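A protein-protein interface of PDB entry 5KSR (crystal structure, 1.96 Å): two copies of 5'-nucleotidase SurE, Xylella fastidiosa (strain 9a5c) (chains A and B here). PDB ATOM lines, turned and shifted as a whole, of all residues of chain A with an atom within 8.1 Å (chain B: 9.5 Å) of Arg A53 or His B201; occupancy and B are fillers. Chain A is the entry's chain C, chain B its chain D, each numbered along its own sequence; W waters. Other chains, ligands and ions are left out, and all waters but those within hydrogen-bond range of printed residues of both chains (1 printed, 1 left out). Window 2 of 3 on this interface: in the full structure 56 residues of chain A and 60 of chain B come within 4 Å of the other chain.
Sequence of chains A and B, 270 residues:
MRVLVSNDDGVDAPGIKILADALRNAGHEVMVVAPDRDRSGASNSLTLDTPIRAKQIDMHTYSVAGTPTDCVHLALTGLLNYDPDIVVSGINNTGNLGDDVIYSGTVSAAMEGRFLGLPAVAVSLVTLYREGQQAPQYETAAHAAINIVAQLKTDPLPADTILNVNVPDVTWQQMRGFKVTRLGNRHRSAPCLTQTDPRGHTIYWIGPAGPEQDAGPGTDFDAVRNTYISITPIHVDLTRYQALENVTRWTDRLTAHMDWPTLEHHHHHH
Of the 15 printed residues of chain A, 5 touch a printed residue of chain B.
Along chain A the printed residues that touch a printed residue of chain B span positions 50 to 79.
Hydrophobic or aromatic side chains of chain B within 4 Å of the printed part of chain A: His B201, Ile B203, Tyr B204 and Trp B205.
Among the printed residues, Asp or Glu carboxylates within 4 Å of a Lys or Arg side-chain nitrogen of the other chain: Arg A53 with Asp B197 (3.3 Å).
The backbone carbonyl oxygen (O) of Arg A53 is in hydrogen-bond range of the backbone NH (N) of Ala A65 (3.2 Å).
OE1 of Gln B195 is in hydrogen-bond range of NE1 of Trp B205, 3.3 Å away.
The backbone NH (N) of Gly B200 sits at hydrogen-bond distance from the side-chain carboxylate (OD1) of Asp B197 (3.3 Å).
O of Gln B195 lies within hydrogen-bond range of N of Ile B203, at 2.9 Å.
N of Arg B199 is in hydrogen-bond range of OD1 of Asp B197, at 2.8 Å.
N of His B201 sits at hydrogen-bond distance from OD1 of Asp B197 (3.4 Å).
Water W1 lies within hydrogen-bond range of O of Thr B202 and O of Ala A54.
The guanidinium group (NH2) of Arg A53 lies close to a ring nitrogen (ND1) of His B201 (3.3 Å).
N of Ile A52 lies within hydrogen-bond range of O of Tyr B204, 3.0 Å away.
The guanidinium group (NH2) of Arg A53 lies within salt-bridge range of the side-chain carboxylate (OD2) of Asp B197, 3.3 Å away.
No position is printed for both chains.
Of the 9 pairs that touch across the chains among the printed residues, none has its exchanged pair printed and touching as well.
C of Thr A50 touches CZ3 of Trp B205, 3.8 Å away.
Ile B203 touches Pro A51 (CD1 to CB, 3.8 Å).
Tyr B204 touches Pro A51 (O to CA, 3.7 Å).
CD of Pro A51 touches CH2 of Trp B205, at 3.7 Å.
Ile B203 touches Ile A52.
Leu A79 touches Tyr B204.
Arg A53 touches two residues of chain B.
His B201 touches just one residue of chain A: Arg A53.
No residue of chain B comes within 4 Å of Ala A54.
No residue of chain B comes within 4 Å of Ala A65.
Of the printed residues of chain A, Asp B197 touches Arg A53 (3.3 Å).
Printed residues of chain B within 4 Å of Leu A79: Tyr B204 (3.9 Å).
Of the printed residues of chain B, Pro A51 touches Ile B203, Tyr B204 and Trp B205.
Printed residues of chain A within 4 Å of Trp B205: Thr A50 and Pro A51.
Gln B195 touches none of the printed residues of chain A.
Pro B198 touches none of the printed residues of chain A.
The nearest printed residue of chain B that does not touch Leu A79 is Thr B194 (7.1 Å).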
ATOM      1  N   ALA A  34      28.023   2.381 -17.447  1.00  0.00           N
ATOM      2  CA  ALA A  34      28.672   1.118 -17.914  1.00  0.00           C
ATOM      3  C   ALA A  34      29.098   0.124 -16.771  1.00  0.00           C
ATOM      4  O   ALA A  34      29.192   0.526 -15.609  1.00  0.00           O
ATOM      5  CB  ALA A  34      29.897   1.464 -18.800  1.00  0.00           C
ATOM      6  N   ASP A  36      30.941  -2.338 -13.915  1.00  0.00           N
ATOM      7  CA  ASP A  36      32.123  -2.231 -13.053  1.00  0.00           C
ATOM      8  C   ASP A  36      33.342  -3.142 -13.412  1.00  0.00           C
ATOM      9  O   ASP A  36      34.450  -2.884 -12.943  1.00  0.00           O
ATOM     10  CB  ASP A  36      31.752  -2.345 -11.553  1.00  0.00           C
ATOM     11  CG  ASP A  36      31.446  -3.780 -11.106  1.00  0.00           C
ATOM     12  OD1 ASP A  36      30.890  -4.578 -11.872  1.00  0.00           O
ATOM     13  OD2 ASP A  36      31.737  -4.097  -9.940  1.00  0.00           O
ATOM     14  N   THR A  50      17.140  -9.847  -7.496  1.00  0.00           N
ATOM     15  CA  THR A  50      17.998  -9.218  -6.468  1.00  0.00           C
ATOM     16  C   THR A  50      18.183  -7.722  -6.807  1.00  0.00           C
ATOM     17  O   THR A  50      18.017  -7.343  -7.976  1.00  0.00           O
ATOM     18  CB  THR A  50      19.430  -9.862  -6.434  1.00  0.00           C
ATOM     19  OG1 THR A  50      20.020  -9.792  -7.737  1.00  0.00           O
ATOM     20  CG2 THR A  50      19.399 -11.331  -6.004  1.00  0.00           C
ATOM     21  N   PRO A  51      18.520  -6.885  -5.799  1.00  0.00           N
ATOM     22  CA  PRO A  51      18.783  -5.442  -6.049  1.00  0.00           C
ATOM     23  C   PRO A  51      20.207  -5.168  -6.600  1.00  0.00           C
ATOM     24  O   PRO A  51      21.078  -6.042  -6.471  1.00  0.00           O
ATOM     25  CB  PRO A  51      18.589  -4.799  -4.668  1.00  0.00           C
ATOM     26  CG  PRO A  51      18.922  -5.891  -3.680  1.00  0.00           C
ATOM     27  CD  PRO A  51      18.502  -7.203  -4.354  1.00  0.00           C
ATOM     28  N   ILE A  52      20.428  -3.977  -7.186  1.00  0.00           N
ATOM     29  CA  ILE A  52      21.664  -3.648  -7.924  1.00  0.00           C
ATOM     30  C   ILE A  52      22.355  -2.381  -7.340  1.00  0.00           C
ATOM     31  O   ILE A  52      21.688  -1.378  -7.127  1.00  0.00           O
ATOM     32  CB  ILE A  52      21.328  -3.370  -9.421  1.00  0.00           C
ATOM     33  CG1 ILE A  52      20.618  -4.567 -10.061  1.00  0.00           C
ATOM     34  CG2 ILE A  52      22.580  -2.993 -10.225  1.00  0.00           C
ATOM     35  CD1 ILE A  52      19.948  -4.250 -11.381  1.00  0.00           C
ATOM     36  N   ARG A  53      23.669  -2.410  -7.097  1.00  0.00           N
ATOM     37  CA  ARG A  53      24.391  -1.191  -6.645  1.00  0.00           C
ATOM     38  C   ARG A  53      24.920  -0.281  -7.792  1.00  0.00           C
ATOM     39  O   ARG A  53      25.315  -0.779  -8.850  1.00  0.00           O
ATOM     40  CB  ARG A  53      25.577  -1.580  -5.755  1.00  0.00           C
ATOM     41  CG  ARG A  53      25.206  -2.120  -4.379  1.00  0.00           C
ATOM     42  CD  ARG A  53      26.464  -2.372  -3.552  1.00  0.00           C
ATOM     43  NE  ARG A  53      26.173  -2.663  -2.148  1.00  0.00           N
ATOM     44  CZ  ARG A  53      27.109  -2.826  -1.219  1.00  0.00           C
ATOM     45  NH1 ARG A  53      28.389  -2.726  -1.543  1.00  0.00           N
ATOM     46  NH2 ARG A  53      26.763  -3.087   0.036  1.00  0.00           N
ATOM     47  N   ALA A  54      24.973   1.039  -7.580  1.00  0.00           N
ATOM     48  CA  ALA A  54      25.612   1.938  -8.569  1.00  0.00           C
ATOM     49  C   ALA A  54      26.226   3.183  -7.930  1.00  0.00           C
ATOM     50  O   ALA A  54      25.678   3.708  -6.945  1.00  0.00           O
ATOM     51  CB  ALA A  54      24.633   2.319  -9.687  1.00  0.00           C
ATOM     52  N   LYS A  55      27.363   3.654  -8.448  1.00  0.00           N
ATOM     53  CA  LYS A  55      28.024   4.838  -7.826  1.00  0.00           C
ATOM     54  C   LYS A  55      28.635   5.854  -8.802  1.00  0.00           C
ATOM     55  O   LYS A  55      29.055   5.490  -9.898  1.00  0.00           O
ATOM     56  CB  LYS A  55      29.105   4.398  -6.836  1.00  0.00           C
ATOM     57  CG  LYS A  55      30.171   3.473  -7.431  1.00  0.00           C
ATOM     58  N   TYR A  62      28.923   7.045 -14.296  1.00  0.00           N
ATOM     59  CA  TYR A  62      28.451   6.070 -13.300  1.00  0.00           C
ATOM     60  C   TYR A  62      28.942   4.614 -13.595  1.00  0.00           C
ATOM     61  O   TYR A  62      28.867   4.157 -14.729  1.00  0.00           O
ATOM     62  CB  TYR A  62      26.907   6.036 -13.281  1.00  0.00           C
ATOM     63  CG  TYR A  62      26.246   7.295 -12.652  1.00  0.00           C
ATOM     64  CD1 TYR A  62      26.043   8.452 -13.400  1.00  0.00           C
ATOM     65  CD2 TYR A  62      25.830   7.300 -11.313  1.00  0.00           C
ATOM     66  CE1 TYR A  62      25.446   9.631 -12.802  1.00  0.00           C
ATOM     67  CE2 TYR A  62      25.236   8.465 -10.715  1.00  0.00           C
ATOM     68  CZ  TYR A  62      25.049   9.609 -11.467  1.00  0.00           C
ATOM     69  OH  TYR A  62      24.464  10.733 -10.875  1.00  0.00           O
ATOM     70  N   SER A  63      29.379   3.903 -12.551  1.00  0.00           N
ATOM     71  CA  SER A  63      29.761   2.472 -12.589  1.00  0.00           C
ATOM     72  C   SER A  63      28.677   1.553 -11.941  1.00  0.00           C
ATOM     73  O   SER A  63      28.279   1.789 -10.791  1.00  0.00           O
ATOM     74  CB  SER A  63      31.104   2.310 -11.844  1.00  0.00           C
ATOM     75  OG  SER A  63      31.487   0.953 -11.663  1.00  0.00           O
ATOM     76  N   VAL A  64      28.232   0.511 -12.664  1.00  0.00           N
ATOM     77  CA  VAL A  64      27.111  -0.364 -12.250  1.00  0.00           C
ATOM     78  C   VAL A  64      27.496  -1.861 -12.064  1.00  0.00           C
ATOM     79  O   VAL A  64      28.060  -2.479 -12.974  1.00  0.00           O
ATOM     80  CB  VAL A  64      25.950  -0.327 -13.313  1.00  0.00           C
ATOM     81  CG1 VAL A  64      24.789  -1.255 -12.913  1.00  0.00           C
ATOM     82  CG2 VAL A  64      25.430   1.102 -13.554  1.00  0.00           C
ATOM     83  N   ALA A  65      27.172  -2.450 -10.905  1.00  0.00           N
ATOM     84  CA  ALA A  65      27.428  -3.900 -10.668  1.00  0.00           C
ATOM     85  C   ALA A  65      26.340  -4.841 -11.236  1.00  0.00           C
ATOM     86  O   ALA A  65      25.555  -5.429 -10.458  1.00  0.00           O
ATOM     87  CB  ALA A  65      27.628  -4.163  -9.181  1.00  0.00           C
ATOM     88  N   GLY A  66      26.319  -4.982 -12.570  1.00  0.00           N
ATOM     89  CA  GLY A  66      25.268  -5.673 -13.335  1.00  0.00           C
ATOM     90  C   GLY A  66      25.537  -5.770 -14.848  1.00  0.00           C
ATOM     91  O   GLY A  66      26.645  -5.426 -15.283  1.00  0.00           O
ATOM     92  N   LEU A  74      18.157   1.129 -16.376  1.00  0.00           N
ATOM     93  CA  LEU A  74      18.170   2.057 -15.248  1.00  0.00           C
ATOM     94  C   LEU A  74      18.328   3.537 -15.671  1.00  0.00           C
ATOM     95  O   LEU A  74      17.607   4.404 -15.157  1.00  0.00           O
ATOM     96  CB  LEU A  74      19.245   1.685 -14.198  1.00  0.00           C
ATOM     97  CG  LEU A  74      18.956   0.452 -13.315  1.00  0.00           C
ATOM     98  CD1 LEU A  74      20.118   0.153 -12.357  1.00  0.00           C
ATOM     99  CD2 LEU A  74      17.652   0.662 -12.495  1.00  0.00           C
ATOM    100  N   LEU A  79      17.108   6.695 -12.980  1.00  0.00           N
ATOM    101  CA  LEU A  79      18.466   6.946 -12.479  1.00  0.00           C
ATOM    102  C   LEU A  79      18.979   8.357 -12.814  1.00  0.00           C
ATOM    103  O   LEU A  79      19.651   8.972 -11.987  1.00  0.00           O
ATOM    104  CB  LEU A  79      19.457   5.869 -12.986  1.00  0.00           C
ATOM    105  CG  LEU A  79      20.935   5.975 -12.520  1.00  0.00           C
ATOM    106  CD1 LEU A  79      21.106   5.781 -10.994  1.00  0.00           C
ATOM    107  CD2 LEU A  79      21.856   5.004 -13.291  1.00  0.00           C
ATOM    108  N   THR B 194      14.010   3.132  -5.418  1.00  0.00           N
ATOM    109  CA  THR B 194      15.207   3.440  -4.624  1.00  0.00           C
ATOM    110  C   THR B 194      15.114   3.061  -3.134  1.00  0.00           C
ATOM    111  O   THR B 194      14.191   3.531  -2.443  1.00  0.00           O
ATOM    112  CB  THR B 194      15.501   4.964  -4.701  1.00  0.00           C
ATOM    113  OG1 THR B 194      15.800   5.327  -6.054  1.00  0.00           O
ATOM    114  CG2 THR B 194      16.665   5.342  -3.808  1.00  0.00           C
ATOM    115  N   GLN B 195      16.081   2.271  -2.631  1.00  0.00           N
ATOM    116  CA  GLN B 195      16.129   1.826  -1.215  1.00  0.00           C
ATOM    117  C   GLN B 195      17.525   1.886  -0.532  1.00  0.00           C
ATOM    118  O   GLN B 195      18.520   2.237  -1.169  1.00  0.00           O
ATOM    119  CB  GLN B 195      15.544   0.403  -1.059  1.00  0.00           C
ATOM    120  CG  GLN B 195      14.020   0.317  -1.208  1.00  0.00           C
ATOM    121  CD  GLN B 195      13.481  -1.123  -1.325  1.00  0.00           C
ATOM    122  OE1 GLN B 195      14.098  -2.090  -0.848  1.00  0.00           O
ATOM    123  NE2 GLN B 195      12.320  -1.264  -1.970  1.00  0.00           N
ATOM    124  N   THR B 196      17.563   1.569   0.775  1.00  0.00           N
ATOM    125  CA  THR B 196      18.809   1.433   1.562  1.00  0.00           C
ATOM    126  C   THR B 196      18.987   0.032   2.220  1.00  0.00           C
ATOM    127  O   THR B 196      18.084  -0.446   2.910  1.00  0.00           O
ATOM    128  CB  THR B 196      18.915   2.531   2.661  1.00  0.00           C
ATOM    129  OG1 THR B 196      18.826   3.838   2.072  1.00  0.00           O
ATOM    130  CG2 THR B 196      20.235   2.412   3.433  1.00  0.00           C
ATOM    131  N   ASP B 197      20.151  -0.609   2.029  1.00  0.00           N
ATOM    132  CA  ASP B 197      20.443  -1.950   2.611  1.00  0.00           C
ATOM    133  C   ASP B 197      20.879  -1.938   4.114  1.00  0.00           C
ATOM    134  O   ASP B 197      20.983  -0.856   4.711  1.00  0.00           O
ATOM    135  CB  ASP B 197      21.378  -2.769   1.665  1.00  0.00           C
ATOM    136  CG  ASP B 197      22.883  -2.532   1.893  1.00  0.00           C
ATOM    137  OD1 ASP B 197      23.309  -1.938   2.896  1.00  0.00           O
ATOM    138  OD2 ASP B 197      23.668  -2.984   1.031  1.00  0.00           O
ATOM    139  N   PRO B 198      21.098  -3.126   4.745  1.00  0.00           N
ATOM    140  CA  PRO B 198      21.429  -3.080   6.183  1.00  0.00           C
ATOM    141  C   PRO B 198      22.789  -2.481   6.576  1.00  0.00           C
ATOM    142  O   PRO B 198      23.013  -2.241   7.758  1.00  0.00           O
ATOM    143  CB  PRO B 198      21.377  -4.557   6.606  1.00  0.00           C
ATOM    144  CG  PRO B 198      20.489  -5.212   5.605  1.00  0.00           C
ATOM    145  CD  PRO B 198      20.797  -4.509   4.317  1.00  0.00           C
ATOM    146  N   ARG B 199      23.681  -2.252   5.623  1.00  0.00           N
ATOM    147  CA  ARG B 199      24.968  -1.625   5.945  1.00  0.00           C
ATOM    148  C   ARG B 199      25.067  -0.140   5.515  1.00  0.00           C
ATOM    149  O   ARG B 199      26.136   0.467   5.601  1.00  0.00           O
ATOM    150  CB  ARG B 199      26.138  -2.454   5.382  1.00  0.00           C
ATOM    151  CG  ARG B 199      26.379  -3.764   6.158  1.00  0.00           C
ATOM    152  CD  ARG B 199      27.278  -4.754   5.421  1.00  0.00           C
ATOM    153  NE  ARG B 199      27.025  -6.130   5.860  1.00  0.00           N
ATOM    154  CZ  ARG B 199      27.737  -6.778   6.785  1.00  0.00           C
ATOM    155  NH1 ARG B 199      28.776  -6.200   7.367  1.00  0.00           N
ATOM    156  NH2 ARG B 199      27.422  -8.021   7.119  1.00  0.00           N
ATOM    157  N   GLY B 200      23.956   0.434   5.053  1.00  0.00           N
ATOM    158  CA  GLY B 200      23.919   1.849   4.704  1.00  0.00           C
ATOM    159  C   GLY B 200      24.126   2.247   3.246  1.00  0.00           C
ATOM    160  O   GLY B 200      24.151   3.443   2.951  1.00  0.00           O
ATOM    161  N   HIS B 201      24.273   1.278   2.339  1.00  0.00           N
ATOM    162  CA  HIS B 201      24.437   1.570   0.903  1.00  0.00           C
ATOM    163  C   HIS B 201      23.101   1.806   0.165  1.00  0.00           C
ATOM    164  O   HIS B 201      22.116   1.091   0.396  1.00  0.00           O
ATOM    165  CB  HIS B 201      25.193   0.437   0.184  1.00  0.00           C
ATOM    166  CG  HIS B 201      26.533   0.120   0.775  1.00  0.00           C
ATOM    167  ND1 HIS B 201      26.685  -0.412   2.039  1.00  0.00           N
ATOM    168  CD2 HIS B 201      27.783   0.248   0.270  1.00  0.00           C
ATOM    169  CE1 HIS B 201      27.970  -0.584   2.293  1.00  0.00           C
ATOM    170  NE2 HIS B 201      28.658  -0.195   1.235  1.00  0.00           N
ATOM    171  N   THR B 202      23.078   2.801  -0.723  1.00  0.00           N
ATOM    172  CA  THR B 202      21.955   3.012  -1.646  1.00  0.00           C
ATOM    173  C   THR B 202      21.823   1.868  -2.696  1.00  0.00           C
ATOM    174  O   THR B 202      22.784   1.604  -3.428  1.00  0.00           O
ATOM    175  CB  THR B 202      22.121   4.368  -2.386  1.00  0.00           C
ATOM    176  OG1 THR B 202      21.976   5.457  -1.449  1.00  0.00           O
ATOM    177  CG2 THR B 202      21.086   4.506  -3.485  1.00  0.00           C
ATOM    178  N   ILE B 203      20.658   1.206  -2.783  1.00  0.00           N
ATOM    179  CA  ILE B 203      20.435   0.123  -3.795  1.00  0.00           C
ATOM    180  C   ILE B 203      19.183   0.386  -4.682  1.00  0.00           C
ATOM    181  O   ILE B 203      18.284   1.144  -4.263  1.00  0.00           O
ATOM    182  CB  ILE B 203      20.282  -1.278  -3.114  1.00  0.00           C
ATOM    183  CG1 ILE B 203      19.182  -1.222  -2.043  1.00  0.00           C
ATOM    184  CG2 ILE B 203      21.587  -1.705  -2.443  1.00  0.00           C
ATOM    185  CD1 ILE B 203      18.689  -2.579  -1.566  1.00  0.00           C
ATOM    186  N   TYR B 204      19.130  -0.244  -5.874  1.00  0.00           N
ATOM    187  CA  TYR B 204      18.042  -0.066  -6.855  1.00  0.00           C
ATOM    188  C   TYR B 204      17.356  -1.390  -7.325  1.00  0.00           C
ATOM    189  O   TYR B 204      18.048  -2.309  -7.776  1.00  0.00           O
ATOM    190  CB  TYR B 204      18.584   0.643  -8.117  1.00  0.00           C
ATOM    191  CG  TYR B 204      19.259   1.991  -7.857  1.00  0.00           C
ATOM    192  CD1 TYR B 204      18.521   3.167  -7.844  1.00  0.00           C
ATOM    193  CD2 TYR B 204      20.633   2.076  -7.632  1.00  0.00           C
ATOM    194  CE1 TYR B 204      19.132   4.407  -7.606  1.00  0.00           C
ATOM    195  CE2 TYR B 204      21.266   3.335  -7.389  1.00  0.00           C
ATOM    196  CZ  TYR B 204      20.499   4.488  -7.376  1.00  0.00           C
ATOM    197  OH  TYR B 204      21.097   5.732  -7.144  1.00  0.00           O
ATOM    198  N   TRP B 205      16.016  -1.454  -7.277  1.00  0.00           N
ATOM    199  CA  TRP B 205      15.238  -2.608  -7.820  1.00  0.00           C
ATOM    200  C   TRP B 205      14.579  -2.276  -9.188  1.00  0.00           C
ATOM    201  O   TRP B 205      14.003  -1.193  -9.363  1.00  0.00           O
ATOM    202  CB  TRP B 205      14.097  -3.047  -6.862  1.00  0.00           C
ATOM    203  CG  TRP B 205      14.418  -3.760  -5.533  1.00  0.00           C
ATOM    204  CD1 TRP B 205      14.593  -3.171  -4.309  1.00  0.00           C
ATOM    205  CD2 TRP B 205      14.509  -5.181  -5.299  1.00  0.00           C
ATOM    206  NE1 TRP B 205      14.813  -4.124  -3.344  1.00  0.00           N
ATOM    207  CE2 TRP B 205      14.774  -5.364  -3.922  1.00  0.00           C
ATOM    208  CE3 TRP B 205      14.423  -6.309  -6.124  1.00  0.00           C
ATOM    209  CZ2 TRP B 205      14.945  -6.630  -3.347  1.00  0.00           C
ATOM    210  CZ3 TRP B 205      14.588  -7.581  -5.547  1.00  0.00           C
ATOM    211  CH2 TRP B 205      14.846  -7.725  -4.173  1.00  0.00           C
HETATM  212  O   HOH W   1      24.834   2.391  -4.835  1.00  0.00           O
